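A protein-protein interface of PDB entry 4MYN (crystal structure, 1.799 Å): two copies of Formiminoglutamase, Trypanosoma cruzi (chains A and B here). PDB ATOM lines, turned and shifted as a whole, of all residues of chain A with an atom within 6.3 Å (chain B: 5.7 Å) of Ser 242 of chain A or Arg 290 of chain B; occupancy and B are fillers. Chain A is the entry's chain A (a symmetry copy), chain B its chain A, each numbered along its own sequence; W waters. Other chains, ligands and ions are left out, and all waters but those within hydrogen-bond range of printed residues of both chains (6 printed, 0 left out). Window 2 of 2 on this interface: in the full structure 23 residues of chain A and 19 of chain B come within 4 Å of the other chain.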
ATOM      1  N   LEU A 240     -23.833 -32.575   4.712  1.00  0.00           N
ATOM      2  CA  LEU A 240     -23.657 -32.275   3.285  1.00  0.00           C
ATOM      3  C   LEU A 240     -24.297 -30.934   2.888  1.00  0.00           C
ATOM      4  O   LEU A 240     -25.382 -30.588   3.364  1.00  0.00           O
ATOM      5  CB  LEU A 240     -24.245 -33.386   2.399  1.00  0.00           C
ATOM      6  CG  LEU A 240     -23.433 -34.676   2.231  1.00  0.00           C
ATOM      7  CD1 LEU A 240     -23.310 -35.412   3.570  1.00  0.00           C
ATOM      8  CD2 LEU A 240     -24.092 -35.549   1.170  1.00  0.00           C
ATOM      9  N   LYS A 241     -23.635 -30.204   1.986  1.00  0.00           N
ATOM     10  CA  LYS A 241     -24.192 -28.949   1.468  1.00  0.00           C
ATOM     11  C   LYS A 241     -25.553 -29.207   0.833  1.00  0.00           C
ATOM     12  O   LYS A 241     -25.739 -30.210   0.153  1.00  0.00           O
ATOM     13  CB  LYS A 241     -23.238 -28.323   0.442  1.00  0.00           C
ATOM     14  CG  LYS A 241     -23.010 -29.195  -0.788  1.00  0.00           C
ATOM     15  CD  LYS A 241     -21.626 -28.948  -1.417  1.00  0.00           C
ATOM     16  CE  LYS A 241     -21.454 -27.511  -1.879  1.00  0.00           C
ATOM     17  NZ  LYS A 241     -20.027 -27.228  -2.276  1.00  0.00           N
ATOM     18  N   SER A 242     -26.503 -28.295   1.041  1.00  0.00           N
ATOM     19  CA  SER A 242     -27.861 -28.533   0.549  1.00  0.00           C
ATOM     20  C   SER A 242     -27.987 -28.443  -0.979  1.00  0.00           C
ATOM     21  O   SER A 242     -29.015 -28.821  -1.536  1.00  0.00           O
ATOM     22  CB  SER A 242     -28.874 -27.601   1.233  1.00  0.00           C
ATOM     23  OG  SER A 242     -28.560 -26.233   0.966  1.00  0.00           O
ATOM     24  N   SER A 243     -26.945 -27.970  -1.660  1.00  0.00           N
ATOM     25  CA  SER A 243     -26.950 -28.040  -3.129  1.00  0.00           C
ATOM     26  C   SER A 243     -26.993 -29.500  -3.615  1.00  0.00           C
ATOM     27  O   SER A 243     -27.636 -29.822  -4.638  1.00  0.00           O
ATOM     28  CB  SER A 243     -25.730 -27.299  -3.709  1.00  0.00           C
ATOM     29  OG  SER A 243     -24.528 -27.848  -3.203  1.00  0.00           O
ATOM     30  N   ASP A 244     -26.289 -30.371  -2.890  1.00  0.00           N
ATOM     31  CA  ASP A 244     -26.272 -31.811  -3.167  1.00  0.00           C
ATOM     32  C   ASP A 244     -27.342 -32.575  -2.387  1.00  0.00           C
ATOM     33  O   ASP A 244     -27.850 -33.596  -2.869  1.00  0.00           O
ATOM     34  CB  ASP A 244     -24.893 -32.419  -2.839  1.00  0.00           C
ATOM     35  CG  ASP A 244     -23.829 -32.043  -3.846  1.00  0.00           C
ATOM     36  OD1 ASP A 244     -24.206 -31.743  -4.993  1.00  0.00           O
ATOM     37  OD2 ASP A 244     -22.621 -32.066  -3.496  1.00  0.00           O
ATOM     38  N   MET A 245     -27.666 -32.089  -1.191  1.00  0.00           N
ATOM     39  CA  MET A 245     -28.468 -32.836  -0.214  1.00  0.00           C
ATOM     40  C   MET A 245     -29.510 -31.920   0.436  1.00  0.00           C
ATOM     41  O   MET A 245     -29.372 -31.509   1.585  1.00  0.00           O
ATOM     42  CB  MET A 245     -27.543 -33.462   0.843  1.00  0.00           C
ATOM     43  CG  MET A 245     -28.135 -34.578   1.701  1.00  0.00           C
ATOM     44  SD  MET A 245     -28.700 -35.926   0.635  1.00  0.00           S
ATOM     45  CE  MET A 245     -28.591 -37.333   1.750  1.00  0.00           C
ATOM     46  N   PRO A 246     -30.559 -31.581  -0.317  1.00  0.00           N
ATOM     47  CA  PRO A 246     -31.506 -30.591   0.206  1.00  0.00           C
ATOM     48  C   PRO A 246     -32.513 -31.222   1.146  1.00  0.00           C
ATOM     49  O   PRO A 246     -33.064 -30.514   1.984  1.00  0.00           O
ATOM     50  CB  PRO A 246     -32.214 -30.087  -1.058  1.00  0.00           C
ATOM     51  CG  PRO A 246     -32.070 -31.200  -2.038  1.00  0.00           C
ATOM     52  CD  PRO A 246     -30.693 -31.760  -1.770  1.00  0.00           C
ATOM     53  N   GLY A 247     -32.735 -32.534   1.008  1.00  0.00           N
ATOM     54  CA  GLY A 247     -33.813 -33.200   1.718  1.00  0.00           C
ATOM     55  C   GLY A 247     -33.449 -33.618   3.127  1.00  0.00           C
ATOM     56  O   GLY A 247     -33.336 -34.820   3.404  1.00  0.00           O
ATOM     57  N   VAL A 248     -33.239 -32.625   3.992  1.00  0.00           N
ATOM     58  CA  VAL A 248     -33.000 -32.820   5.419  1.00  0.00           C
ATOM     59  C   VAL A 248     -33.755 -31.770   6.226  1.00  0.00           C
ATOM     60  O   VAL A 248     -34.198 -30.744   5.695  1.00  0.00           O
ATOM     61  CB  VAL A 248     -31.484 -32.721   5.774  1.00  0.00           C
ATOM     62  CG1 VAL A 248     -30.717 -33.813   5.084  1.00  0.00           C
ATOM     63  CG2 VAL A 248     -30.930 -31.351   5.404  1.00  0.00           C
ATOM     64  N   PRO A 251     -31.221 -27.966   6.408  1.00  0.00           N
ATOM     65  CA  PRO A 251     -30.372 -27.902   5.207  1.00  0.00           C
ATOM     66  C   PRO A 251     -29.157 -27.013   5.408  1.00  0.00           C
ATOM     67  O   PRO A 251     -29.267 -25.913   5.956  1.00  0.00           O
ATOM     68  CB  PRO A 251     -31.306 -27.311   4.143  1.00  0.00           C
ATOM     69  CG  PRO A 251     -32.680 -27.713   4.610  1.00  0.00           C
ATOM     70  CD  PRO A 251     -32.614 -27.581   6.115  1.00  0.00           C
ATOM     71  N   ALA A 252     -28.000 -27.496   4.966  1.00  0.00           N
ATOM     72  CA  ALA A 252     -26.751 -26.786   5.193  1.00  0.00           C
ATOM     73  C   ALA A 252     -26.464 -25.866   4.007  1.00  0.00           C
ATOM     74  O   ALA A 252     -26.673 -26.258   2.870  1.00  0.00           O
ATOM     75  CB  ALA A 252     -25.619 -27.779   5.360  1.00  0.00           C
ATOM     76  N   ALA A 253     -25.993 -24.650   4.262  1.00  0.00           N
ATOM     77  CA  ALA A 253     -25.600 -23.749   3.163  1.00  0.00           C
ATOM     78  C   ALA A 253     -24.289 -24.214   2.541  1.00  0.00           C
ATOM     79  O   ALA A 253     -24.164 -24.347   1.307  1.00  0.00           O
ATOM     80  CB  ALA A 253     -25.460 -22.306   3.669  1.00  0.00           C
ATOM     81  N   VAL A 254     -23.311 -24.440   3.414  1.00  0.00           N
ATOM     82  CA  VAL A 254     -22.041 -25.032   3.052  1.00  0.00           C
ATOM     83  C   VAL A 254     -21.967 -26.401   3.734  1.00  0.00           C
ATOM     84  O   VAL A 254     -22.765 -26.710   4.636  1.00  0.00           O
ATOM     85  CB  VAL A 254     -20.847 -24.163   3.490  1.00  0.00           C
ATOM     86  CG1 VAL A 254     -20.792 -22.820   2.703  1.00  0.00           C
ATOM     87  CG2 VAL A 254     -20.922 -23.867   4.982  1.00  0.00           C
ATOM     88  N   GLY A 255     -21.012 -27.217   3.326  1.00  0.00           N
ATOM     89  CA  GLY A 255     -20.894 -28.545   3.904  1.00  0.00           C
ATOM     90  C   GLY A 255     -20.202 -29.508   2.964  1.00  0.00           C
ATOM     91  O   GLY A 255     -19.605 -29.099   1.954  1.00  0.00           O
ATOM     92  N   LEU A 256     -20.256 -30.794   3.301  1.00  0.00           N
ATOM     93  CA  LEU A 256     -19.581 -31.807   2.499  1.00  0.00           C
ATOM     94  C   LEU A 256     -20.249 -31.966   1.146  1.00  0.00           C
ATOM     95  O   LEU A 256     -21.466 -31.904   1.062  1.00  0.00           O
ATOM     96  CB  LEU A 256     -19.627 -33.156   3.221  1.00  0.00           C
ATOM     97  CG  LEU A 256     -18.873 -33.159   4.552  1.00  0.00           C
ATOM     98  CD1 LEU A 256     -19.209 -34.434   5.342  1.00  0.00           C
ATOM     99  CD2 LEU A 256     -17.366 -33.029   4.293  1.00  0.00           C
ATOM    100  N   ARG A 290     -33.779 -36.486  -5.187  1.00  0.00           N
ATOM    101  CA  ARG A 290     -32.329 -36.356  -5.260  1.00  0.00           C
ATOM    102  C   ARG A 290     -31.672 -36.832  -3.964  1.00  0.00           C
ATOM    103  O   ARG A 290     -30.635 -37.509  -3.977  1.00  0.00           O
ATOM    104  CB  ARG A 290     -31.946 -34.911  -5.586  1.00  0.00           C
ATOM    105  CG  ARG A 290     -32.363 -34.487  -6.997  1.00  0.00           C
ATOM    106  CD  ARG A 290     -32.072 -33.000  -7.237  1.00  0.00           C
ATOM    107  NE  ARG A 290     -30.647 -32.736  -7.047  1.00  0.00           N
ATOM    108  CZ  ARG A 290     -30.132 -31.799  -6.259  1.00  0.00           C
ATOM    109  NH1 ARG A 290     -30.913 -30.977  -5.564  1.00  0.00           N
ATOM    110  NH2 ARG A 290     -28.814 -31.681  -6.184  1.00  0.00           N
ATOM    111  N   SER B 242     -26.502 -20.632  -8.880  1.00  0.00           N
ATOM    112  CA  SER B 242     -27.858 -20.935  -8.416  1.00  0.00           C
ATOM    113  C   SER B 242     -27.983 -22.303  -7.728  1.00  0.00           C
ATOM    114  O   SER B 242     -29.006 -22.592  -7.113  1.00  0.00           O
ATOM    115  CB  SER B 242     -28.880 -20.804  -9.555  1.00  0.00           C
ATOM    116  OG  SER B 242     -28.579 -21.721 -10.610  1.00  0.00           O
ATOM    117  N   SER B 243     -26.945 -23.133  -7.806  1.00  0.00           N
ATOM    118  CA  SER B 243     -26.947 -24.370  -7.011  1.00  0.00           C
ATOM    119  C   SER B 243     -26.975 -24.061  -5.504  1.00  0.00           C
ATOM    120  O   SER B 243     -27.614 -24.784  -4.708  1.00  0.00           O
ATOM    121  CB  SER B 243     -25.733 -25.247  -7.374  1.00  0.00           C
ATOM    122  OG  SER B 243     -24.527 -24.539  -7.162  1.00  0.00           O
ATOM    123  N   ASP B 244     -26.264 -23.000  -5.117  1.00  0.00           N
ATOM    124  CA  ASP B 244     -26.233 -22.520  -3.732  1.00  0.00           C
ATOM    125  C   ASP B 244     -27.297 -21.459  -3.451  1.00  0.00           C
ATOM    126  O   ASP B 244     -27.794 -21.364  -2.322  1.00  0.00           O
ATOM    127  CB  ASP B 244     -24.848 -21.937  -3.382  1.00  0.00           C
ATOM    128  CG  ASP B 244     -23.788 -23.001  -3.214  1.00  0.00           C
ATOM    129  OD1 ASP B 244     -24.165 -24.143  -2.897  1.00  0.00           O
ATOM    130  OD2 ASP B 244     -22.580 -22.691  -3.380  1.00  0.00           O
ATOM    131  N   MET B 245     -27.626 -20.665  -4.468  1.00  0.00           N
ATOM    132  CA  MET B 245     -28.423 -19.442  -4.302  1.00  0.00           C
ATOM    133  C   MET B 245     -29.474 -19.333  -5.412  1.00  0.00           C
ATOM    134  O   MET B 245     -29.341 -18.544  -6.342  1.00  0.00           O
ATOM    135  CB  MET B 245     -27.493 -18.217  -4.297  1.00  0.00           C
ATOM    136  CG  MET B 245     -28.076 -16.914  -3.754  1.00  0.00           C
ATOM    137  SD  MET B 245     -28.626 -17.162  -2.049  1.00  0.00           S
ATOM    138  CE  MET B 245     -28.505 -15.493  -1.389  1.00  0.00           C
ATOM    139  N   PRO B 246     -30.525 -20.152  -5.319  1.00  0.00           N
ATOM    140  CA  PRO B 246     -31.482 -20.189  -6.429  1.00  0.00           C
ATOM    141  C   PRO B 246     -32.485 -19.056  -6.344  1.00  0.00           C
ATOM    142  O   PRO B 246     -33.044 -18.682  -7.372  1.00  0.00           O
ATOM    143  CB  PRO B 246     -32.193 -21.534  -6.227  1.00  0.00           C
ATOM    144  CG  PRO B 246     -32.038 -21.827  -4.775  1.00  0.00           C
ATOM    145  CD  PRO B 246     -30.656 -21.319  -4.436  1.00  0.00           C
ATOM    146  N   GLU B 287     -37.210 -18.885  -4.589  1.00  0.00           N
ATOM    147  CA  GLU B 287     -36.939 -19.961  -3.622  1.00  0.00           C
ATOM    148  C   GLU B 287     -36.862 -19.349  -2.214  1.00  0.00           C
ATOM    149  O   GLU B 287     -36.154 -18.374  -2.009  1.00  0.00           O
ATOM    150  CB  GLU B 287     -35.657 -20.727  -3.987  1.00  0.00           C
ATOM    151  CG  GLU B 287     -35.429 -22.010  -3.159  1.00  0.00           C
ATOM    152  CD  GLU B 287     -34.860 -21.743  -1.767  1.00  0.00           C
ATOM    153  OE1 GLU B 287     -34.070 -20.781  -1.622  1.00  0.00           O
ATOM    154  OE2 GLU B 287     -35.178 -22.514  -0.827  1.00  0.00           O
ATOM    155  N   GLU B 288     -37.608 -19.894  -1.256  1.00  0.00           N
ATOM    156  CA  GLU B 288     -37.856 -19.152  -0.015  1.00  0.00           C
ATOM    157  C   GLU B 288     -37.094 -19.558   1.240  1.00  0.00           C
ATOM    158  O   GLU B 288     -37.195 -18.879   2.259  1.00  0.00           O
ATOM    159  CB  GLU B 288     -39.352 -19.145   0.310  1.00  0.00           C
ATOM    160  CG  GLU B 288     -39.912 -20.487   0.727  1.00  0.00           C
ATOM    161  CD  GLU B 288     -41.380 -20.402   1.133  1.00  0.00           C
ATOM    162  OE1 GLU B 288     -42.187 -21.211   0.627  1.00  0.00           O
ATOM    163  OE2 GLU B 288     -41.728 -19.528   1.960  1.00  0.00           O
ATOM    164  N   TYR B 289     -36.332 -20.640   1.187  1.00  0.00           N
ATOM    165  CA  TYR B 289     -35.763 -21.201   2.414  1.00  0.00           C
ATOM    166  C   TYR B 289     -34.242 -21.234   2.389  1.00  0.00           C
ATOM    167  O   TYR B 289     -33.573 -20.657   3.252  1.00  0.00           O
ATOM    168  CB  TYR B 289     -36.295 -22.624   2.648  1.00  0.00           C
ATOM    169  CG  TYR B 289     -36.168 -23.090   4.087  1.00  0.00           C
ATOM    170  CD1 TYR B 289     -37.211 -22.901   4.987  1.00  0.00           C
ATOM    171  CD2 TYR B 289     -35.010 -23.717   4.546  1.00  0.00           C
ATOM    172  CE1 TYR B 289     -37.108 -23.313   6.307  1.00  0.00           C
ATOM    173  CE2 TYR B 289     -34.896 -24.140   5.874  1.00  0.00           C
ATOM    174  CZ  TYR B 289     -35.945 -23.931   6.745  1.00  0.00           C
ATOM    175  OH  TYR B 289     -35.852 -24.336   8.061  1.00  0.00           O
ATOM    176  N   ARG B 290     -33.692 -21.904   1.391  1.00  0.00           N
ATOM    177  CA  ARG B 290     -32.244 -22.037   1.304  1.00  0.00           C
ATOM    178  C   ARG B 290     -31.584 -20.680   1.061  1.00  0.00           C
ATOM    179  O   ARG B 290     -30.541 -20.357   1.645  1.00  0.00           O
ATOM    180  CB  ARG B 290     -31.874 -23.044   0.211  1.00  0.00           C
ATOM    181  CG  ARG B 290     -32.294 -24.477   0.553  1.00  0.00           C
ATOM    182  CD  ARG B 290     -32.017 -25.429  -0.616  1.00  0.00           C
ATOM    183  NE  ARG B 290     -30.595 -25.403  -0.953  1.00  0.00           N
ATOM    184  CZ  ARG B 290     -30.089 -25.189  -2.162  1.00  0.00           C
ATOM    185  NH1 ARG B 290     -30.878 -24.996  -3.215  1.00  0.00           N
ATOM    186  NH2 ARG B 290     -28.772 -25.189  -2.314  1.00  0.00           N
ATOM    187  N   SER B 291     -32.195 -19.881   0.196  1.00  0.00           N
ATOM    188  CA  SER B 291     -31.555 -18.661  -0.254  1.00  0.00           C
ATOM    189  C   SER B 291     -31.519 -17.582   0.826  1.00  0.00           C
ATOM    190  O   SER B 291     -30.487 -16.955   1.031  1.00  0.00           O
ATOM    191  CB  SER B 291     -32.174 -18.167  -1.571  1.00  0.00           C
ATOM    192  OG  SER B 291     -32.088 -19.200  -2.562  1.00  0.00           O
ATOM    193  N   PRO B 292     -32.641 -17.361   1.531  1.00  0.00           N
ATOM    194  CA  PRO B 292     -32.543 -16.345   2.584  1.00  0.00           C
ATOM    195  C   PRO B 292     -31.559 -16.751   3.673  1.00  0.00           C
ATOM    196  O   PRO B 292     -30.922 -15.898   4.288  1.00  0.00           O
ATOM    197  CB  PRO B 292     -33.971 -16.282   3.142  1.00  0.00           C
ATOM    198  CG  PRO B 292     -34.842 -16.715   1.948  1.00  0.00           C
ATOM    199  CD  PRO B 292     -34.034 -17.818   1.318  1.00  0.00           C
ATOM    200  N   ARG B 293     -31.431 -18.051   3.910  1.00  0.00           N
ATOM    201  CA  ARG B 293     -30.436 -18.536   4.867  1.00  0.00           C
ATOM    202  C   ARG B 293     -29.014 -18.163   4.436  1.00  0.00           C
ATOM    203  O   ARG B 293     -28.199 -17.694   5.254  1.00  0.00           O
ATOM    204  CB  ARG B 293     -30.578 -20.051   5.079  1.00  0.00           C
ATOM    205  CG  ARG B 293     -31.842 -20.454   5.856  1.00  0.00           C
ATOM    206  CD  ARG B 293     -32.001 -21.988   5.924  1.00  0.00           C
ATOM    207  NE  ARG B 293     -30.999 -22.586   6.797  1.00  0.00           N
ATOM    208  CZ  ARG B 293     -31.204 -22.913   8.070  1.00  0.00           C
ATOM    209  NH1 ARG B 293     -32.395 -22.728   8.629  1.00  0.00           N
ATOM    210  NH2 ARG B 293     -30.218 -23.448   8.782  1.00  0.00           N
ATOM    211  N   VAL B 294     -28.710 -18.369   3.159  1.00  0.00           N
ATOM    212  CA  VAL B 294     -27.419 -17.937   2.618  1.00  0.00           C
ATOM    213  C   VAL B 294     -27.218 -16.434   2.805  1.00  0.00           C
ATOM    214  O   VAL B 294     -26.141 -15.989   3.210  1.00  0.00           O
ATOM    215  CB  VAL B 294     -27.257 -18.331   1.132  1.00  0.00           C
ATOM    216  CG1 VAL B 294     -25.990 -17.677   0.528  1.00  0.00           C
ATOM    217  CG2 VAL B 294     -27.248 -19.898   0.995  1.00  0.00           C
ATOM    218  N   ALA B 295     -28.249 -15.640   2.507  1.00  0.00           N
ATOM    219  CA  ALA B 295     -28.153 -14.197   2.682  1.00  0.00           C
ATOM    220  C   ALA B 295     -27.852 -13.823   4.130  1.00  0.00           C
ATOM    221  O   ALA B 295     -26.992 -12.987   4.393  1.00  0.00           O
ATOM    222  CB  ALA B 295     -29.460 -13.513   2.230  1.00  0.00           C
HETATM  223  O   HOH W   1     -20.881 -24.742  -3.656  1.00  0.00           O
HETATM  224  O   HOH W   2     -25.803 -25.191  -0.686  1.00  0.00           O
HETATM  225  O   HOH W   3     -27.806 -23.083  -0.034  1.00  0.00           O
HETATM  226  O   HOH W   4     -29.449 -27.315  -6.121  1.00  0.00           O
HETATM  227  O   HOH W   5     -23.215 -25.904  -5.137  1.00  0.00           O
HETATM  228  O   HOH W   6     -22.327 -24.601  -0.672  1.00  0.00           O
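The side-chain hydroxyl of Ser 242 of chain A lies within hydrogen-bond range of the guanidinium group of Arg 290 of chain B, at 2.9 Å. The backbone NH (N) of Ser 243 of chain A sits close to the guanidinium group (NH2) of Arg 290 of chain B, at 3.4 Å.
Water W1 bridges the side-chain carboxylate of Asp 244 of chain B (2.7 Å) and the side-chain amino group of Lys 241 of chain A (3.0 Å). Water W6 lies within hydrogen-bond range of O of Ala 253 of chain A (2.7 Å) and OD1 of Asp 244 of chain B (2.9 Å). Water W2 lies within hydrogen-bond range of the backbone carbonyl oxygen (O) of Ala 253 of chain A (2.7 Å), the side-chain carboxylate (OD1) of Asp 244 of chain B (2.9 Å), the backbone NH (N) of Ser 243 of chain A (3.2 Å), the side-chain hydroxyl (OG) of Ser 242 of chain A (3.4 Å) and the guanidinium group (NH2) of Arg 290 of chain B (3.4 Å). Water W5 lies within hydrogen-bond range of the side-chain hydroxyl of Ser 243 of chain B (2.8 Å), the side-chain carboxylate of Asp 244 of chain B (3.0 Å) and the side-chain hydroxyl of Ser 243 of chain A (3.0 Å). Water W3 lies within hydrogen-bond range of O of Asp 244 of chain B (2.9 Å), NH2 of Arg 290 of chain B (3.3 Å) and OG of Ser 242 of chain A (3.4 Å). Water W4 lies within hydrogen-bond range of O of Ser 243 of chain B (3.4 Å) and O of Ser 243 of chain A (3.4 Å).
Of the 16 printed residues of chain A, 3 touch a printed residue of chain B. Printed residues of chain A that touch a printed residue of chain B: Ser 242, Ser 243 and Pro 251. Printed residues of chain B that touch a printed residue of chain A: Ser 243, Asp 244, Arg 290 and Arg 293. Among the printed residues, 5 pairs touch across the chains. Among the printed residues, no Asp or Glu carboxylate lies within 4 Å of a Lys or Arg side-chain nitrogen of the other chain.
Ser 242 of chain A touches just one residue of chain B: Arg 290 (2.9 Å). Arg 290 of chain B touches just these residues of chain A: Ser 242 (2.9 Å) and Ser 243 (3.4 Å). Of the printed residues of chain A, Arg 293 of chain B touches Pro 251 (3.8 Å). Printed residues of chain A within 4 Å of Asp 244 of chain B: Ser 243 (3.6 Å). Of the printed residues of chain A, Ser 243 of chain B touches Ser 243. Printed residues of chain B within 4 Å of Ser 243 of chain A: Ser 243, Asp 244 and Arg 290. Val 248 of chain A touches none of the printed residues of chain B. Gly 247 of chain A touches none of the printed residues of chain B.
Ser 242 of chain A touches Arg 290 of chain B, but with the chains exchanged Arg 290 of chain A does not touch Ser 242 of chain B (8.7 Å). Ser 243 of chain A touches its own counterpart, Ser 243 of chain B. Ser 243 of chain A touches Asp 244 of chain B, but with the chains exchanged Asp 244 of chain A does not touch Ser 243 of chain B (6.0 Å). Ser 243 of chain A touches Arg 290 of chain B, but with the chains exchanged Arg 290 of chain A does not touch Ser 243 of chain B (7.1 Å). Of the 5 pairs that touch across the chains among the printed residues, 1 has its exchanged pair printed and touching as well.
Among the printed residues, merely in contact across the chains: Ser 243 of chain A with Ser 243 of chain B (3.3 Å), Ser 243 of chain A with Asp 244 of chain B (3.6 Å) and Pro 251 of chain A with Arg 293 of chain B (3.8 Å).
The backbone carbonyl oxygen of Ser 243 of chain B is in hydrogen-bond range of the guanidinium group of Arg 290 of chain B (2.7 Å). The side-chain carboxylate (OE2) of Glu 287 of chain B sits at hydrogen-bond distance from the backbone NH (N) of Arg 290 of chain B (2.7 Å). The side-chain hydroxyl (OG) of Ser 242 of chain A is in hydrogen-bond range of the backbone carbonyl oxygen (O) of Ala 252 of chain A, 2.7 Å away. O of Ser 243 of chain A lies within hydrogen-bond range of NH2 of Arg 290 of chain A.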
